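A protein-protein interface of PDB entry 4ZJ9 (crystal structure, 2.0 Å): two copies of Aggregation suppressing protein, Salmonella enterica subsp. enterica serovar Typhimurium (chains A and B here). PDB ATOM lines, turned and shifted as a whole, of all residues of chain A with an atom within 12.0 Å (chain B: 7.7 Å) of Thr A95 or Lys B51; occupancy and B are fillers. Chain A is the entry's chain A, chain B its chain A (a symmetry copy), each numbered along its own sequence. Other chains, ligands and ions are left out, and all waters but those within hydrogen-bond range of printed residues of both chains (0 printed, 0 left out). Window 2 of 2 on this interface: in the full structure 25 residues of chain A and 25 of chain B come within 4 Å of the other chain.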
ATOM      1  N   THR A  90       9.115 -18.356 -10.240  1.00  0.00           N
ATOM      2  CA  THR A  90       9.818 -17.285 -10.824  1.00  0.00           C
ATOM      3  C   THR A  90      11.266 -17.857 -10.990  1.00  0.00           C
ATOM      4  O   THR A  90      11.748 -18.613 -10.133  1.00  0.00           O
ATOM      5  CB  THR A  90       9.729 -16.093  -9.841  1.00  0.00           C
ATOM      6  OG1 THR A  90      10.608 -15.041 -10.252  1.00  0.00           O
ATOM      7  CG2 THR A  90      10.096 -16.512  -8.404  1.00  0.00           C
ATOM      8  N   VAL A  91      11.937 -17.542 -12.093  1.00  0.00           N
ATOM      9  CA  VAL A  91      13.366 -17.877 -12.234  1.00  0.00           C
ATOM     10  C   VAL A  91      14.218 -17.020 -11.307  1.00  0.00           C
ATOM     11  O   VAL A  91      14.132 -15.801 -11.377  1.00  0.00           O
ATOM     12  CB  VAL A  91      13.873 -17.707 -13.673  1.00  0.00           C
ATOM     13  CG1 VAL A  91      15.398 -17.911 -13.695  1.00  0.00           C
ATOM     14  CG2 VAL A  91      13.129 -18.667 -14.625  1.00  0.00           C
ATOM     15  N   GLU A  92      15.055 -17.649 -10.487  1.00  0.00           N
ATOM     16  CA  GLU A  92      15.818 -16.943  -9.491  1.00  0.00           C
ATOM     17  C   GLU A  92      17.300 -17.173  -9.642  1.00  0.00           C
ATOM     18  O   GLU A  92      17.805 -18.303  -9.507  1.00  0.00           O
ATOM     19  CB  GLU A  92      15.314 -17.325  -8.131  1.00  0.00           C
ATOM     20  CG  GLU A  92      13.899 -16.798  -7.985  1.00  0.00           C
ATOM     21  CD  GLU A  92      13.405 -16.754  -6.572  1.00  0.00           C
ATOM     22  OE1 GLU A  92      13.770 -17.660  -5.806  1.00  0.00           O
ATOM     23  OE2 GLU A  92      12.640 -15.821  -6.253  1.00  0.00           O
ATOM     24  N   ASP A  93      18.004 -16.089  -9.954  1.00  0.00           N
ATOM     25  CA  ASP A  93      19.379 -16.143 -10.242  1.00  0.00           C
ATOM     26  C   ASP A  93      20.097 -16.296  -8.936  1.00  0.00           C
ATOM     27  O   ASP A  93      20.130 -15.391  -8.145  1.00  0.00           O
ATOM     28  CB  ASP A  93      19.841 -14.882 -11.038  1.00  0.00           C
ATOM     29  CG  ASP A  93      21.294 -15.011 -11.530  1.00  0.00           C
ATOM     30  OD1 ASP A  93      22.006 -15.899 -11.024  1.00  0.00           O
ATOM     31  OD2 ASP A  93      21.752 -14.189 -12.344  1.00  0.00           O
ATOM     32  N   GLN A  94      20.707 -17.438  -8.719  1.00  0.00           N
ATOM     33  CA  GLN A  94      21.253 -17.778  -7.403  1.00  0.00           C
ATOM     34  C   GLN A  94      22.508 -16.961  -7.072  1.00  0.00           C
ATOM     35  O   GLN A  94      22.914 -16.906  -5.908  1.00  0.00           O
ATOM     36  CB  GLN A  94      21.517 -19.293  -7.258  1.00  0.00           C
ATOM     37  CG  GLN A  94      20.320 -20.214  -7.512  1.00  0.00           C
ATOM     38  CD  GLN A  94      19.141 -19.971  -6.559  1.00  0.00           C
ATOM     39  OE1 GLN A  94      19.219 -20.303  -5.375  1.00  0.00           O
ATOM     40  NE2 GLN A  94      18.042 -19.405  -7.080  1.00  0.00           N
ATOM     41  N   THR A  95      23.111 -16.337  -8.086  1.00  0.00           N
ATOM     42  CA  THR A  95      24.167 -15.377  -7.861  1.00  0.00           C
ATOM     43  C   THR A  95      23.702 -14.106  -7.092  1.00  0.00           C
ATOM     44  O   THR A  95      24.442 -13.616  -6.207  1.00  0.00           O
ATOM     45  CB  THR A  95      24.871 -14.980  -9.185  1.00  0.00           C
ATOM     46  OG1 THR A  95      26.165 -14.438  -8.899  1.00  0.00           O
ATOM     47  CG2 THR A  95      24.103 -13.961  -9.980  1.00  0.00           C
ATOM     48  N   HIS A  96      22.490 -13.607  -7.431  1.00  0.00           N
ATOM     49  CA  HIS A  96      21.841 -12.461  -6.760  1.00  0.00           C
ATOM     50  C   HIS A  96      21.482 -12.758  -5.331  1.00  0.00           C
ATOM     51  O   HIS A  96      21.174 -11.868  -4.572  1.00  0.00           O
ATOM     52  CB  HIS A  96      20.519 -12.073  -7.424  1.00  0.00           C
ATOM     53  CG  HIS A  96      20.665 -11.456  -8.775  1.00  0.00           C
ATOM     54  ND1 HIS A  96      21.871 -11.359  -9.438  1.00  0.00           N
ATOM     55  CD2 HIS A  96      19.733 -10.948  -9.615  1.00  0.00           C
ATOM     56  CE1 HIS A  96      21.681 -10.781 -10.611  1.00  0.00           C
ATOM     57  NE2 HIS A  96      20.392 -10.532 -10.749  1.00  0.00           N
ATOM     58  N   TRP A  97      21.421 -14.027  -4.982  1.00  0.00           N
ATOM     59  CA  TRP A  97      21.088 -14.424  -3.639  1.00  0.00           C
ATOM     60  C   TRP A  97      22.395 -14.627  -2.966  1.00  0.00           C
ATOM     61  O   TRP A  97      23.212 -15.434  -3.400  1.00  0.00           O
ATOM     62  CB  TRP A  97      20.235 -15.688  -3.626  1.00  0.00           C
ATOM     63  CG  TRP A  97      18.849 -15.322  -4.076  1.00  0.00           C
ATOM     64  CD1 TRP A  97      18.374 -15.255  -5.359  1.00  0.00           C
ATOM     65  CD2 TRP A  97      17.808 -14.844  -3.238  1.00  0.00           C
ATOM     66  NE1 TRP A  97      17.078 -14.807  -5.371  1.00  0.00           N
ATOM     67  CE2 TRP A  97      16.696 -14.562  -4.076  1.00  0.00           C
ATOM     68  CE3 TRP A  97      17.693 -14.649  -1.854  1.00  0.00           C
ATOM     69  CZ2 TRP A  97      15.494 -14.088  -3.571  1.00  0.00           C
ATOM     70  CZ3 TRP A  97      16.509 -14.204  -1.363  1.00  0.00           C
ATOM     71  CH2 TRP A  97      15.413 -13.929  -2.212  1.00  0.00           C
ATOM     72  N   ILE A  98      22.616 -13.809  -1.955  1.00  0.00           N
ATOM     73  CA  ILE A  98      23.769 -13.924  -1.099  1.00  0.00           C
ATOM     74  C   ILE A  98      23.421 -14.837   0.077  1.00  0.00           C
ATOM     75  O   ILE A  98      24.220 -15.745   0.488  1.00  0.00           O
ATOM     76  CB  ILE A  98      24.193 -12.547  -0.604  1.00  0.00           C
ATOM     77  CG1 ILE A  98      24.694 -11.703  -1.784  1.00  0.00           C
ATOM     78  CG2 ILE A  98      25.241 -12.731   0.468  1.00  0.00           C
ATOM     79  CD1 ILE A  98      25.029 -10.245  -1.447  1.00  0.00           C
ATOM     80  N   TYR A  99      22.213 -14.633   0.601  1.00  0.00           N
ATOM     81  CA  TYR A  99      21.748 -15.371   1.760  1.00  0.00           C
ATOM     82  C   TYR A  99      20.241 -15.358   1.755  1.00  0.00           C
ATOM     83  O   TYR A  99      19.622 -14.330   1.466  1.00  0.00           O
ATOM     84  CB  TYR A  99      22.269 -14.758   3.034  1.00  0.00           C
ATOM     85  CG  TYR A  99      21.688 -15.399   4.231  1.00  0.00           C
ATOM     86  CD1 TYR A  99      21.995 -16.720   4.547  1.00  0.00           C
ATOM     87  CD2 TYR A  99      20.799 -14.737   5.020  1.00  0.00           C
ATOM     88  CE1 TYR A  99      21.404 -17.341   5.618  1.00  0.00           C
ATOM     89  CE2 TYR A  99      20.236 -15.351   6.122  1.00  0.00           C
ATOM     90  CZ  TYR A  99      20.537 -16.636   6.408  1.00  0.00           C
ATOM     91  OH  TYR A  99      19.974 -17.217   7.500  1.00  0.00           O
ATOM     92  N   ARG A 100      19.644 -16.511   2.036  1.00  0.00           N
ATOM     93  CA  ARG A 100      18.176 -16.593   1.997  1.00  0.00           C
ATOM     94  C   ARG A 100      17.705 -17.275   3.224  1.00  0.00           C
ATOM     95  O   ARG A 100      17.715 -18.511   3.335  1.00  0.00           O
ATOM     96  CB  ARG A 100      17.719 -17.295   0.764  1.00  0.00           C
ATOM     97  CG  ARG A 100      16.230 -17.379   0.623  1.00  0.00           C
ATOM     98  CD  ARG A 100      15.850 -17.965  -0.724  1.00  0.00           C
ATOM     99  NE  ARG A 100      14.584 -17.398  -1.192  1.00  0.00           N
ATOM    100  CZ  ARG A 100      14.206 -17.350  -2.462  1.00  0.00           C
ATOM    101  NH1 ARG A 100      14.991 -17.837  -3.432  1.00  0.00           N
ATOM    102  NH2 ARG A 100      13.039 -16.792  -2.757  1.00  0.00           N
ATOM    103  N   GLY A 101      17.361 -16.441   4.194  1.00  0.00           N
ATOM    104  CA  GLY A 101      16.950 -16.907   5.463  1.00  0.00           C
ATOM    105  C   GLY A 101      15.463 -16.943   5.562  1.00  0.00           C
ATOM    106  O   GLY A 101      14.954 -17.518   6.477  1.00  0.00           O
ATOM    107  N   LEU B  49      19.451 -11.520   1.882  1.00  0.00           N
ATOM    108  CA  LEU B  49      20.349 -10.505   1.349  1.00  0.00           C
ATOM    109  C   LEU B  49      20.544 -10.783  -0.088  1.00  0.00           C
ATOM    110  O   LEU B  49      20.955 -11.904  -0.476  1.00  0.00           O
ATOM    111  CB  LEU B  49      21.689 -10.514   2.119  1.00  0.00           C
ATOM    112  CG  LEU B  49      22.668  -9.413   1.720  1.00  0.00           C
ATOM    113  CD1 LEU B  49      22.152  -8.009   2.045  1.00  0.00           C
ATOM    114  CD2 LEU B  49      23.965  -9.740   2.455  1.00  0.00           C
ATOM    115  N   GLN B  50      20.187  -9.820  -0.905  1.00  0.00           N
ATOM    116  CA  GLN B  50      20.377  -9.978  -2.313  1.00  0.00           C
ATOM    117  C   GLN B  50      21.294  -8.928  -2.876  1.00  0.00           C
ATOM    118  O   GLN B  50      21.452  -7.858  -2.313  1.00  0.00           O
ATOM    119  CB  GLN B  50      19.023  -9.821  -3.032  1.00  0.00           C
ATOM    120  CG  GLN B  50      18.052 -10.929  -2.728  1.00  0.00           C
ATOM    121  CD  GLN B  50      16.604 -10.506  -3.061  1.00  0.00           C
ATOM    122  OE1 GLN B  50      15.893 -10.049  -2.213  1.00  0.00           O
ATOM    123  NE2 GLN B  50      16.229 -10.597  -4.324  1.00  0.00           N
ATOM    124  N   LYS B  51      21.898  -9.268  -4.007  1.00  0.00           N
ATOM    125  CA  LYS B  51      22.786  -8.406  -4.798  1.00  0.00           C
ATOM    126  C   LYS B  51      22.008  -8.106  -6.139  1.00  0.00           C
ATOM    127  O   LYS B  51      21.847  -9.010  -6.963  1.00  0.00           O
ATOM    128  CB  LYS B  51      24.115  -9.176  -4.983  1.00  0.00           C
ATOM    129  CG  LYS B  51      25.293  -8.442  -5.599  1.00  0.00           C
ATOM    130  CD  LYS B  51      26.608  -9.274  -5.470  1.00  0.00           C
ATOM    131  CE  LYS B  51      26.496 -10.676  -6.123  1.00  0.00           C
ATOM    132  NZ  LYS B  51      27.777 -11.454  -6.305  1.00  0.00           N
ATOM    133  N   ARG B  52      21.472  -6.889  -6.311  1.00  0.00           N
ATOM    134  CA  ARG B  52      20.714  -6.533  -7.534  1.00  0.00           C
ATOM    135  C   ARG B  52      21.677  -6.381  -8.706  1.00  0.00           C
ATOM    136  O   ARG B  52      21.326  -6.642  -9.849  1.00  0.00           O
ATOM    137  CB  ARG B  52      19.924  -5.234  -7.354  1.00  0.00           C
ATOM    138  CG  ARG B  52      18.918  -5.227  -6.210  1.00  0.00           C
ATOM    139  N   ASP B  53      22.884  -5.916  -8.383  1.00  0.00           N
ATOM    140  CA  ASP B  53      24.068  -5.961  -9.247  1.00  0.00           C
ATOM    141  C   ASP B  53      25.275  -5.649  -8.346  1.00  0.00           C
ATOM    142  O   ASP B  53      25.131  -5.672  -7.130  1.00  0.00           O
ATOM    143  CB  ASP B  53      23.944  -4.966 -10.390  1.00  0.00           C
ATOM    144  CG  ASP B  53      23.685  -3.571  -9.907  1.00  0.00           C
ATOM    145  OD1 ASP B  53      22.503  -3.139  -9.903  1.00  0.00           O
ATOM    146  OD2 ASP B  53      24.674  -2.922  -9.513  1.00  0.00           O
ATOM    147  N   ALA B  54      26.452  -5.368  -8.902  1.00  0.00           N
ATOM    148  CA  ALA B  54      27.681  -5.323  -8.085  1.00  0.00           C
ATOM    149  C   ALA B  54      27.787  -4.134  -7.130  1.00  0.00           C
ATOM    150  O   ALA B  54      28.460  -4.228  -6.110  1.00  0.00           O
ATOM    151  CB  ALA B  54      28.913  -5.392  -8.972  1.00  0.00           C
ATOM    152  N   ASN B  55      27.116  -3.032  -7.462  1.00  0.00           N
ATOM    153  CA  ASN B  55      27.108  -1.817  -6.627  1.00  0.00           C
ATOM    154  C   ASN B  55      25.800  -1.618  -5.797  1.00  0.00           C
ATOM    155  O   ASN B  55      25.586  -0.550  -5.222  1.00  0.00           O
ATOM    156  CB  ASN B  55      27.392  -0.579  -7.509  1.00  0.00           C
ATOM    157  N   ASN B  56      24.941  -2.643  -5.742  1.00  0.00           N
ATOM    158  CA  ASN B  56      23.640  -2.591  -5.035  1.00  0.00           C
ATOM    159  C   ASN B  56      23.363  -3.861  -4.188  1.00  0.00           C
ATOM    160  O   ASN B  56      23.697  -4.975  -4.573  1.00  0.00           O
ATOM    161  CB  ASN B  56      22.454  -2.410  -6.014  1.00  0.00           C
ATOM    162  CG  ASN B  56      22.546  -1.146  -6.849  1.00  0.00           C
ATOM    163  OD1 ASN B  56      22.890  -1.196  -8.027  1.00  0.00           O
ATOM    164  ND2 ASN B  56      22.215  -0.015  -6.254  1.00  0.00           N
ATOM    165  N   TYR B  57      22.737  -3.666  -3.040  1.00  0.00           N
ATOM    166  CA  TYR B  57      22.271  -4.767  -2.240  1.00  0.00           C
ATOM    167  C   TYR B  57      20.831  -4.484  -1.787  1.00  0.00           C
ATOM    168  O   TYR B  57      20.420  -3.376  -1.706  1.00  0.00           O
ATOM    169  CB  TYR B  57      23.185  -4.967  -1.034  1.00  0.00           C
ATOM    170  CG  TYR B  57      24.631  -5.219  -1.384  1.00  0.00           C
ATOM    171  CD1 TYR B  57      25.542  -4.161  -1.542  1.00  0.00           C
ATOM    172  CD2 TYR B  57      25.093  -6.506  -1.566  1.00  0.00           C
ATOM    173  CE1 TYR B  57      26.868  -4.403  -1.889  1.00  0.00           C
ATOM    174  CE2 TYR B  57      26.412  -6.758  -1.895  1.00  0.00           C
ATOM    175  CZ  TYR B  57      27.297  -5.718  -2.066  1.00  0.00           C
ATOM    176  OH  TYR B  57      28.584  -6.043  -2.409  1.00  0.00           O
ATOM    177  N   LEU B  58      20.072  -5.537  -1.534  1.00  0.00           N
ATOM    178  CA  LEU B  58      18.744  -5.440  -0.928  1.00  0.00           C
ATOM    179  C   LEU B  58      18.716  -6.345   0.262  1.00  0.00           C
ATOM    180  O   LEU B  58      18.913  -7.542   0.145  1.00  0.00           O
ATOM    181  CB  LEU B  58      17.619  -5.768  -1.882  1.00  0.00           C
ATOM    182  CG  LEU B  58      16.217  -5.666  -1.224  1.00  0.00           C
ATOM    183  CD1 LEU B  58      15.792  -4.222  -0.984  1.00  0.00           C
ATOM    184  CD2 LEU B  58      15.151  -6.406  -2.041  1.00  0.00           C
ATOM    185  N   LEU B  59      18.487  -5.745   1.418  1.00  0.00           N
ATOM    186  CA  LEU B  59      18.335  -6.479   2.649  1.00  0.00           C
ATOM    187  C   LEU B  59      16.850  -6.565   2.941  1.00  0.00           C
ATOM    188  O   LEU B  59      16.119  -5.551   2.932  1.00  0.00           O
ATOM    189  CB  LEU B  59      19.041  -5.724   3.787  1.00  0.00           C
ATOM    190  CG  LEU B  59      18.756  -6.263   5.169  1.00  0.00           C
ATOM    191  CD1 LEU B  59      19.379  -7.636   5.336  1.00  0.00           C
ATOM    192  CD2 LEU B  59      19.304  -5.241   6.154  1.00  0.00           C
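The backbone NH (N) of Thr A95 sits close to the side-chain carboxylate (OD1) of Asp A93 (3.2 Å). O of Gln B50 is in hydrogen-bond range of N of Leu B58 (2.8 Å).
Printed residues of chain A that touch a printed residue of chain B: Thr A95, His A96, Trp A97, Ile A98 and Tyr A99. Hydrophobic or aromatic side chains of chain A that line the printed part of chain B: His A96, Trp A97 and Ile A98. Of the 11 printed residues of chain B, 4 touch a printed residue of chain A. Among the printed residues, 9 pairs touch across the chains.
No position is printed for both chains. Of the 9 pairs that touch across the chains among the printed residues, none has its exchanged pair printed and touching as well.
Among the printed residues, merely in contact across the chains: His A96 with Gln B50, Thr A95 with Lys B51, Trp A97 with Gln B50, Ile A98 with Tyr B57, Ile A98 with Lys B51 and Trp A97 with Leu B49.
The backbone carbonyl oxygen (O) of His A96 is in hydrogen-bond range of the backbone NH (N) of Lys B51, at 2.8 Å. The backbone NH (N) of Ile A98 is in hydrogen-bond range of the backbone carbonyl oxygen (O) of Leu B49, 2.9 Å away. The backbone NH (N) of Leu B49 lies within hydrogen-bond range of the backbone carbonyl oxygen (O) of Tyr A99 (2.8 Å).
Of chain B, only Lys B51 comes within 4 Å of Thr A95. Lys B51 touches three residues of chain A. Leu B49 touches just these residues of chain A: Trp A97 (3.96 Å), Ile A98 (2.9 Å) and Tyr A99 (2.8 Å). Arg B52 touches none of the printed residues of chain A. Asp B53 touches none of the printed residues of chain A. Of chain A, only Ile A98 comes within 4 Å of Tyr B57. Of the printed residues of chain B, Tyr A99 touches Leu B49. Printed residues of chain B within 4 Å of Trp A97: Leu B49 and Gln B50. Of the printed residues of chain B, Ile A98 touches Leu B49 (2.9 Å), Lys B51 (3.8 Å) and Tyr B57 (3.7 Å). Asn B55 touches none of the printed residues of chain A. Asn B56 touches none of the printed residues of chain A. The nearest residue of chain B that does not touch Thr A95 is Gln B50 (6.6 Å). The nearest printed residue of chain B that does not touch Tyr A99 is Gln B50 (5.1 Å).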
